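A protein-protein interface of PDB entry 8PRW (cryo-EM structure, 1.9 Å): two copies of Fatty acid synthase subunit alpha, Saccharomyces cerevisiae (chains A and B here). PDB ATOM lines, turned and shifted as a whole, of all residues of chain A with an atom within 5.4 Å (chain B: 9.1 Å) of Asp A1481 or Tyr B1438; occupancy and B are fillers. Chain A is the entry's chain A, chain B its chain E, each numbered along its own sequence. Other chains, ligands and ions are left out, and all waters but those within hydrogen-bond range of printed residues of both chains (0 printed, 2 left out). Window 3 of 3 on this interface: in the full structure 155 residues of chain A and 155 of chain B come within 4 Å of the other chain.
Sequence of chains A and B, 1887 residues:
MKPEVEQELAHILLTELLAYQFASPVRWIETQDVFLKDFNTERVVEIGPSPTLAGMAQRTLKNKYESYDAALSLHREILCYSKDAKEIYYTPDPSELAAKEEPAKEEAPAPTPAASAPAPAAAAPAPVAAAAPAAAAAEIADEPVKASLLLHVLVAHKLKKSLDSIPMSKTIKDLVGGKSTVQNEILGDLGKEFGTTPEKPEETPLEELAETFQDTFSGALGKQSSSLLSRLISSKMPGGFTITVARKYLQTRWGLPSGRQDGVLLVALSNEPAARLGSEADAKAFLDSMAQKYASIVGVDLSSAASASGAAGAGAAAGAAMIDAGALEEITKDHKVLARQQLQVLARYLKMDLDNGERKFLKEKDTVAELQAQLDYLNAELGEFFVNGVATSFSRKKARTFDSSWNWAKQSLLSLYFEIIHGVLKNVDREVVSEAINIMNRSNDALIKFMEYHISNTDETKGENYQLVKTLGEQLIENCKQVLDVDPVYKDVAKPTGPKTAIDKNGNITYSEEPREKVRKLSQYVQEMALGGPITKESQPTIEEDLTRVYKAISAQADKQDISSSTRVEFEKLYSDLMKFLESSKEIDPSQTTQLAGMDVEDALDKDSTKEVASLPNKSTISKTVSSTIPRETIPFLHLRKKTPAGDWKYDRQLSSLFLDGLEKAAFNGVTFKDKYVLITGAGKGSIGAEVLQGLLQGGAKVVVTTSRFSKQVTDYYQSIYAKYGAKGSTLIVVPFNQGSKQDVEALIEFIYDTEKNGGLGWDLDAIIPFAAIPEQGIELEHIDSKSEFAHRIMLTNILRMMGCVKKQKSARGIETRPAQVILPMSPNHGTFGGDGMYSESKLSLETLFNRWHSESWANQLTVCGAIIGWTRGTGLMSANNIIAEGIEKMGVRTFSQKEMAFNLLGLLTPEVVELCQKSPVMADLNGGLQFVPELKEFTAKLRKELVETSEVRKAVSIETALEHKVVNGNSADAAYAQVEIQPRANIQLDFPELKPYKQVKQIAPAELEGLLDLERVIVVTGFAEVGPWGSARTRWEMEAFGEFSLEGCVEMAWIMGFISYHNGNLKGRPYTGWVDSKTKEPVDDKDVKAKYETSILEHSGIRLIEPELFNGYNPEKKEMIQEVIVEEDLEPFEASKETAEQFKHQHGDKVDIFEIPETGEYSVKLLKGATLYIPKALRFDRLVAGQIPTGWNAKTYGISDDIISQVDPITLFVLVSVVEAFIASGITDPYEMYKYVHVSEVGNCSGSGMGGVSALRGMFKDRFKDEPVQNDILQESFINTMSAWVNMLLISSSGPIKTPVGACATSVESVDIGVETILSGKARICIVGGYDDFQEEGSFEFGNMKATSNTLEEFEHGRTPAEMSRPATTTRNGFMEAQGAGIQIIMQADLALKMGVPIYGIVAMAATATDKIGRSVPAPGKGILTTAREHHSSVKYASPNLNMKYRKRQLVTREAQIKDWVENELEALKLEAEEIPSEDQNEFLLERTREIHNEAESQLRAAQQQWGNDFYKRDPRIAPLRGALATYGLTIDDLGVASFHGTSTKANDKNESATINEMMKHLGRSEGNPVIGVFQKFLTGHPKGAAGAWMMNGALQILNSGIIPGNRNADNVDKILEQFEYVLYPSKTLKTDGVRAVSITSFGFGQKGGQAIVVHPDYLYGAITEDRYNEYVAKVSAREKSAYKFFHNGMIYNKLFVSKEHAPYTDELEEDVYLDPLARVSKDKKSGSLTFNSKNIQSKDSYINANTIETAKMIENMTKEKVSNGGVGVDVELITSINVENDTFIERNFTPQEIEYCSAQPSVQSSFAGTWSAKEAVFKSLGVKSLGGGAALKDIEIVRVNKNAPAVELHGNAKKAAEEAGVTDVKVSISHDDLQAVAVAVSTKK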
ATOM      1  N   ILE A1477       8.779 -11.925   8.550  1.00  0.00           N
ATOM      2  CA  ILE A1477       8.003 -13.203   8.539  1.00  0.00           C
ATOM      3  C   ILE A1477       8.828 -14.229   7.761  1.00  0.00           C
ATOM      4  O   ILE A1477       9.350 -13.907   6.695  1.00  0.00           O
ATOM      5  CB  ILE A1477       6.588 -12.991   7.938  1.00  0.00           C
ATOM      6  CG1 ILE A1477       5.748 -11.994   8.747  1.00  0.00           C
ATOM      7  CG2 ILE A1477       5.845 -14.304   7.743  1.00  0.00           C
ATOM      8  CD1 ILE A1477       5.257 -12.499  10.085  1.00  0.00           C
ATOM      9  N   PRO A1478       8.995 -15.482   8.260  1.00  0.00           N
ATOM     10  CA  PRO A1478       9.653 -16.540   7.486  1.00  0.00           C
ATOM     11  C   PRO A1478       8.967 -16.785   6.130  1.00  0.00           C
ATOM     12  O   PRO A1478       7.749 -16.754   6.083  1.00  0.00           O
ATOM     13  CB  PRO A1478       9.581 -17.794   8.375  1.00  0.00           C
ATOM     14  CG  PRO A1478       8.608 -17.447   9.492  1.00  0.00           C
ATOM     15  CD  PRO A1478       8.605 -15.938   9.605  1.00  0.00           C
ATOM     16  N   SER A1479       9.766 -17.026   5.082  1.00  0.00           N
ATOM     17  CA  SER A1479       9.387 -16.965   3.641  1.00  0.00           C
ATOM     18  C   SER A1479       8.211 -17.895   3.306  1.00  0.00           C
ATOM     19  O   SER A1479       7.418 -17.521   2.417  1.00  0.00           O
ATOM     20  CB  SER A1479      10.576 -17.262   2.755  1.00  0.00           C
ATOM     21  OG  SER A1479      11.282 -18.404   3.219  1.00  0.00           O
ATOM     22  N   GLU A1480       8.107 -19.053   3.969  1.00  0.00           N
ATOM     23  CA  GLU A1480       7.031 -20.063   3.734  1.00  0.00           C
ATOM     24  C   GLU A1480       5.673 -19.517   4.215  1.00  0.00           C
ATOM     25  O   GLU A1480       4.665 -19.815   3.546  1.00  0.00           O
ATOM     26  CB  GLU A1480       7.379 -21.419   4.370  1.00  0.00           C
ATOM     27  CG  GLU A1480       7.537 -21.420   5.892  1.00  0.00           C
ATOM     28  CD  GLU A1480       8.959 -21.270   6.417  1.00  0.00           C
ATOM     29  OE1 GLU A1480       9.675 -20.367   5.937  1.00  0.00           O
ATOM     30  OE2 GLU A1480       9.348 -22.052   7.310  1.00  0.00           O
ATOM     31  N   ASP A1481       5.658 -18.732   5.304  1.00  0.00           N
ATOM     32  CA  ASP A1481       4.440 -18.175   5.960  1.00  0.00           C
ATOM     33  C   ASP A1481       4.111 -16.764   5.437  1.00  0.00           C
ATOM     34  O   ASP A1481       3.076 -16.205   5.866  1.00  0.00           O
ATOM     35  CB  ASP A1481       4.611 -18.120   7.481  1.00  0.00           C
ATOM     36  CG  ASP A1481       4.928 -19.452   8.145  1.00  0.00           C
ATOM     37  OD1 ASP A1481       4.686 -20.503   7.513  1.00  0.00           O
ATOM     38  OD2 ASP A1481       5.401 -19.428   9.301  1.00  0.00           O
ATOM     39  N   GLN A1482       4.934 -16.216   4.540  1.00  0.00           N
ATOM     40  CA  GLN A1482       4.860 -14.809   4.063  1.00  0.00           C
ATOM     41  C   GLN A1482       3.639 -14.648   3.152  1.00  0.00           C
ATOM     42  O   GLN A1482       2.974 -13.611   3.245  1.00  0.00           O
ATOM     43  CB  GLN A1482       6.140 -14.431   3.314  1.00  0.00           C
ATOM     44  CG  GLN A1482       6.563 -12.989   3.507  1.00  0.00           C
ATOM     45  CD  GLN A1482       7.928 -12.737   2.916  1.00  0.00           C
ATOM     46  OE1 GLN A1482       8.087 -12.634   1.701  1.00  0.00           O
ATOM     47  NE2 GLN A1482       8.927 -12.641   3.779  1.00  0.00           N
ATOM     48  N   ASN A1483       3.367 -15.652   2.317  1.00  0.00           N
ATOM     49  CA  ASN A1483       2.201 -15.675   1.403  1.00  0.00           C
ATOM     50  C   ASN A1483       0.918 -15.499   2.231  1.00  0.00           C
ATOM     51  O   ASN A1483       0.184 -14.536   1.947  1.00  0.00           O
ATOM     52  CB  ASN A1483       2.160 -16.951   0.565  1.00  0.00           C
ATOM     53  CG  ASN A1483       0.973 -16.997  -0.369  1.00  0.00           C
ATOM     54  OD1 ASN A1483       0.194 -17.946  -0.336  1.00  0.00           O
ATOM     55  ND2 ASN A1483       0.818 -15.961  -1.184  1.00  0.00           N
ATOM     56  N   GLU A1484       0.684 -16.361   3.228  1.00  0.00           N
ATOM     57  CA  GLU A1484      -0.588 -16.408   4.002  1.00  0.00           C
ATOM     58  C   GLU A1484      -0.741 -15.086   4.764  1.00  0.00           C
ATOM     59  O   GLU A1484      -1.848 -14.502   4.712  1.00  0.00           O
ATOM     60  CB  GLU A1484      -0.651 -17.635   4.916  1.00  0.00           C
ATOM     61  CG  GLU A1484      -1.939 -17.750   5.736  1.00  0.00           C
ATOM     62  CD  GLU A1484      -3.271 -17.650   4.989  1.00  0.00           C
ATOM     63  OE1 GLU A1484      -3.345 -18.073   3.810  1.00  0.00           O
ATOM     64  OE2 GLU A1484      -4.247 -17.156   5.596  1.00  0.00           O
ATOM     65  N   PHE A1485       0.337 -14.605   5.379  1.00  0.00           N
ATOM     66  CA  PHE A1485       0.385 -13.320   6.121  1.00  0.00           C
ATOM     67  C   PHE A1485      -0.054 -12.161   5.219  1.00  0.00           C
ATOM     68  O   PHE A1485      -0.898 -11.356   5.668  1.00  0.00           O
ATOM     69  CB  PHE A1485       1.782 -13.065   6.671  1.00  0.00           C
ATOM     70  CG  PHE A1485       1.993 -11.725   7.323  1.00  0.00           C
ATOM     71  CD1 PHE A1485       1.565 -11.489   8.615  1.00  0.00           C
ATOM     72  CD2 PHE A1485       2.682 -10.719   6.668  1.00  0.00           C
ATOM     73  CE1 PHE A1485       1.820 -10.279   9.247  1.00  0.00           C
ATOM     74  CE2 PHE A1485       2.910  -9.501   7.284  1.00  0.00           C
ATOM     75  CZ  PHE A1485       2.456  -9.273   8.565  1.00  0.00           C
ATOM     76  N   LEU A1486       0.489 -12.068   4.012  1.00  0.00           N
ATOM     77  CA  LEU A1486       0.210 -10.945   3.075  1.00  0.00           C
ATOM     78  C   LEU A1486      -1.228 -11.037   2.558  1.00  0.00           C
ATOM     79  O   LEU A1486      -1.846  -9.987   2.413  1.00  0.00           O
ATOM     80  CB  LEU A1486       1.202 -10.969   1.910  1.00  0.00           C
ATOM     81  CG  LEU A1486       2.622 -10.559   2.291  1.00  0.00           C
ATOM     82  CD1 LEU A1486       3.580 -10.795   1.140  1.00  0.00           C
ATOM     83  CD2 LEU A1486       2.665  -9.111   2.752  1.00  0.00           C
ATOM     84  N   GLU A1488      -3.831 -12.337   4.216  1.00  0.00           N
ATOM     85  CA  GLU A1488      -4.725 -11.940   5.337  1.00  0.00           C
ATOM     86  C   GLU A1488      -4.638 -10.431   5.489  1.00  0.00           C
ATOM     87  O   GLU A1488      -5.697  -9.788   5.579  1.00  0.00           O
ATOM     88  CB  GLU A1488      -4.363 -12.623   6.661  1.00  0.00           C
ATOM     89  CG  GLU A1488      -4.676 -14.108   6.656  1.00  0.00           C
ATOM     90  CD  GLU A1488      -4.506 -14.879   7.968  1.00  0.00           C
ATOM     91  OE1 GLU A1488      -4.355 -14.239   9.044  1.00  0.00           O
ATOM     92  OE2 GLU A1488      -4.579 -16.129   7.915  1.00  0.00           O
ATOM     93  N   SER B1434     -11.703 -19.078   7.561  1.00  0.00           N
ATOM     94  CA  SER B1434     -10.831 -19.740   6.530  1.00  0.00           C
ATOM     95  C   SER B1434      -9.374 -19.315   6.682  1.00  0.00           C
ATOM     96  O   SER B1434      -8.498 -20.147   6.412  1.00  0.00           O
ATOM     97  CB  SER B1434     -11.292 -19.474   5.110  1.00  0.00           C
ATOM     98  OG  SER B1434     -11.115 -18.115   4.740  1.00  0.00           O
ATOM     99  N   SER B1435      -9.141 -18.086   7.137  1.00  0.00           N
ATOM    100  CA  SER B1435      -7.841 -17.373   7.103  1.00  0.00           C
ATOM    101  C   SER B1435      -7.606 -16.680   8.441  1.00  0.00           C
ATOM    102  O   SER B1435      -7.892 -15.474   8.528  1.00  0.00           O
ATOM    103  CB  SER B1435      -7.885 -16.373   5.953  1.00  0.00           C
ATOM    104  OG  SER B1435      -8.599 -16.933   4.850  1.00  0.00           O
ATOM    105  N   VAL B1436      -7.133 -17.410   9.450  1.00  0.00           N
ATOM    106  CA  VAL B1436      -7.009 -16.887  10.844  1.00  0.00           C
ATOM    107  C   VAL B1436      -5.635 -17.201  11.435  1.00  0.00           C
ATOM    108  O   VAL B1436      -5.506 -17.155  12.672  1.00  0.00           O
ATOM    109  CB  VAL B1436      -8.153 -17.433  11.729  1.00  0.00           C
ATOM    110  CG1 VAL B1436      -9.481 -16.836  11.304  1.00  0.00           C
ATOM    111  CG2 VAL B1436      -8.207 -18.954  11.733  1.00  0.00           C
ATOM    112  N   LYS B1437      -4.629 -17.411  10.589  1.00  0.00           N
ATOM    113  CA  LYS B1437      -3.250 -17.720  11.041  1.00  0.00           C
ATOM    114  C   LYS B1437      -2.709 -16.519  11.824  1.00  0.00           C
ATOM    115  O   LYS B1437      -2.059 -16.739  12.858  1.00  0.00           O
ATOM    116  CB  LYS B1437      -2.366 -18.076   9.846  1.00  0.00           C
ATOM    117  CG  LYS B1437      -1.107 -18.852  10.209  1.00  0.00           C
ATOM    118  CD  LYS B1437      -0.205 -19.139   9.011  1.00  0.00           C
ATOM    119  CE  LYS B1437       0.717 -20.340   9.140  1.00  0.00           C
ATOM    120  NZ  LYS B1437       1.037 -20.708  10.545  1.00  0.00           N
ATOM    121  N   TYR B1438      -3.043 -15.299  11.401  1.00  0.00           N
ATOM    122  CA  TYR B1438      -2.529 -14.045  12.009  1.00  0.00           C
ATOM    123  C   TYR B1438      -3.670 -13.206  12.569  1.00  0.00           C
ATOM    124  O   TYR B1438      -4.729 -13.111  11.925  1.00  0.00           O
ATOM    125  CB  TYR B1438      -1.706 -13.275  10.978  1.00  0.00           C
ATOM    126  CG  TYR B1438      -0.521 -14.085  10.532  1.00  0.00           C
ATOM    127  CD1 TYR B1438       0.589 -14.209  11.353  1.00  0.00           C
ATOM    128  CD2 TYR B1438      -0.559 -14.830   9.363  1.00  0.00           C
ATOM    129  CE1 TYR B1438       1.665 -15.003  10.991  1.00  0.00           C
ATOM    130  CE2 TYR B1438       0.512 -15.627   8.988  1.00  0.00           C
ATOM    131  CZ  TYR B1438       1.629 -15.706   9.802  1.00  0.00           C
ATOM    132  OH  TYR B1438       2.691 -16.476   9.435  1.00  0.00           O
ATOM    133  N   ALA B1439      -3.447 -12.622  13.744  1.00  0.00           N
ATOM    134  CA  ALA B1439      -4.397 -11.710  14.414  1.00  0.00           C
ATOM    135  C   ALA B1439      -4.656 -10.517  13.483  1.00  0.00           C
ATOM    136  O   ALA B1439      -3.695 -10.025  12.847  1.00  0.00           O
ATOM    137  CB  ALA B1439      -3.840 -11.281  15.751  1.00  0.00           C
ATOM    138  N   SER B1440      -5.923 -10.130  13.338  1.00  0.00           N
ATOM    139  CA  SER B1440      -6.341  -8.906  12.611  1.00  0.00           C
ATOM    140  C   SER B1440      -5.920  -7.690  13.428  1.00  0.00           C
ATOM    141  O   SER B1440      -6.318  -7.576  14.588  1.00  0.00           O
ATOM    142  CB  SER B1440      -7.822  -8.881  12.371  1.00  0.00           C
ATOM    143  OG  SER B1440      -8.191  -7.693  11.674  1.00  0.00           O
ATOM    144  N   PRO B1441      -5.171  -6.721  12.853  1.00  0.00           N
ATOM    145  CA  PRO B1441      -4.932  -5.447  13.531  1.00  0.00           C
ATOM    146  C   PRO B1441      -6.227  -4.724  13.936  1.00  0.00           C
ATOM    147  O   PRO B1441      -6.221  -3.985  14.894  1.00  0.00           O
ATOM    148  CB  PRO B1441      -4.172  -4.609  12.494  1.00  0.00           C
ATOM    149  CG  PRO B1441      -3.521  -5.654  11.603  1.00  0.00           C
ATOM    150  CD  PRO B1441      -4.543  -6.767  11.523  1.00  0.00           C
ATOM    151  N   ASN B1442      -7.309  -4.976  13.217  1.00  0.00           N
ATOM    152  CA  ASN B1442      -8.625  -4.335  13.451  1.00  0.00           C
ATOM    153  C   ASN B1442      -9.176  -4.733  14.820  1.00  0.00           C
ATOM    154  O   ASN B1442      -9.928  -3.929  15.393  1.00  0.00           O
ATOM    155  CB  ASN B1442      -9.588  -4.662  12.313  1.00  0.00           C
ATOM    156  CG  ASN B1442     -10.576  -3.551  12.065  1.00  0.00           C
ATOM    157  OD1 ASN B1442     -10.229  -2.372  12.134  1.00  0.00           O
ATOM    158  ND2 ASN B1442     -11.801  -3.938  11.758  1.00  0.00           N
ATOM    159  N   LEU B1443      -8.761  -5.872  15.374  1.00  0.00           N
ATOM    160  CA  LEU B1443      -9.183  -6.320  16.724  1.00  0.00           C
ATOM    161  C   LEU B1443      -8.325  -5.709  17.817  1.00  0.00           C
ATOM    162  O   LEU B1443      -8.681  -5.870  18.993  1.00  0.00           O
ATOM    163  CB  LEU B1443      -9.140  -7.842  16.836  1.00  0.00           C
ATOM    164  CG  LEU B1443     -10.479  -8.548  16.746  1.00  0.00           C
ATOM    165  CD1 LEU B1443     -10.282 -10.004  17.141  1.00  0.00           C
ATOM    166  CD2 LEU B1443     -11.543  -7.872  17.616  1.00  0.00           C
ATOM    167  N   ARG B1518     -14.254 -11.390   9.576  1.00  0.00           N
ATOM    168  CA  ARG B1518     -13.470 -12.102  10.591  1.00  0.00           C
ATOM    169  C   ARG B1518     -13.851 -11.695  12.010  1.00  0.00           C
ATOM    170  O   ARG B1518     -13.340 -12.327  12.932  1.00  0.00           O
ATOM    171  CB  ARG B1518     -11.992 -11.797  10.373  1.00  0.00           C
ATOM    172  CG  ARG B1518     -11.438 -12.521   9.156  1.00  0.00           C
ATOM    173  CD  ARG B1518      -9.943 -12.288   9.061  1.00  0.00           C
ATOM    174  NE  ARG B1518      -9.230 -12.869  10.189  1.00  0.00           N
ATOM    175  CZ  ARG B1518      -7.911 -12.806  10.385  1.00  0.00           C
ATOM    176  NH1 ARG B1518      -7.132 -12.183   9.514  1.00  0.00           N
ATOM    177  NH2 ARG B1518      -7.383 -13.383  11.455  1.00  0.00           N
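The side-chain carboxylate of Glu A1488 lies within hydrogen-bond range of the backbone NH of Val B1436, 3.2 Å away.
The side-chain carboxylate of Glu A1488 lies close to the backbone carbonyl oxygen of Ser B1435 (3.4 Å).
The backbone NH of Lys B1437 sits at hydrogen-bond distance from the side-chain carboxylate of Glu A1488.
The backbone NH (N) of Tyr B1438 sits at hydrogen-bond distance from the side-chain carboxylate (OE1) of Glu A1488.
The side-chain carboxylate of Glu A1488 is in salt-bridge range of the guanidinium group of Arg B1518, 3.5 Å away.
OE2 of Glu A1484 lies close to OE2 of Glu A1488.
The backbone carbonyl oxygen of Tyr B1438 lies within hydrogen-bond range of the guanidinium group of Arg B1518, 2.7 Å away.
OG of Ser B1434 lies within hydrogen-bond range of OG of Ser B1435, 2.8 Å away.
The backbone carbonyl oxygen (O) of Ser B1435 lies close to the guanidinium group (NE) of Arg B1518 (3.4 Å).
Among the printed residues, merely in contact across the chains: Asp A1481 with Tyr B1438 (3.2 Å), Phe A1485 with Tyr B1438 (3.7 Å), Glu A1484 with Ser B1435 (3.7 Å) and Glu A1484 with Lys B1437 (3.96 Å).
No residue of chain B comes within 4 Å of Glu A1480.
Asp A1481 touches one residue of chain B.
Printed residues of chain B within 4 Å of Phe A1485: Tyr B1438.
Printed residues of chain B within 4 Å of Glu A1488: Ser B1435, Val B1436, Lys B1437, Tyr B1438 and Arg B1518.
Of the printed residues of chain A, Val B1436 touches Glu A1488.
Of chain A, only Asp A1481 (3.2 Å), Phe A1485 (3.7 Å) and Glu A1488 (2.9 Å) come within 4 Å of Tyr B1438.
Of the printed residues of chain A, Arg B1518 touches Glu A1488 (3.5 Å).
The nearest residue of chain A that does not touch Tyr B1438 is Ile A1477 (4.2 Å).
The nearest printed residue of chain A that does not touch Arg B1518 is Glu A1484 (7.0 Å).
Printed residues of chain A that touch a printed residue of chain B: Asp A1481, Glu A1484, Phe A1485 and Glu A1488.
Among the printed residues, Asp or Glu carboxylates within 4 Å of a Lys or Arg side-chain nitrogen of the other chain: Glu A1488 with Arg B1518 (3.5 Å).
No position is printed for both chains.
Of the 9 pairs that touch across the chains among the printed residues, none has its exchanged pair printed and touching as well.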
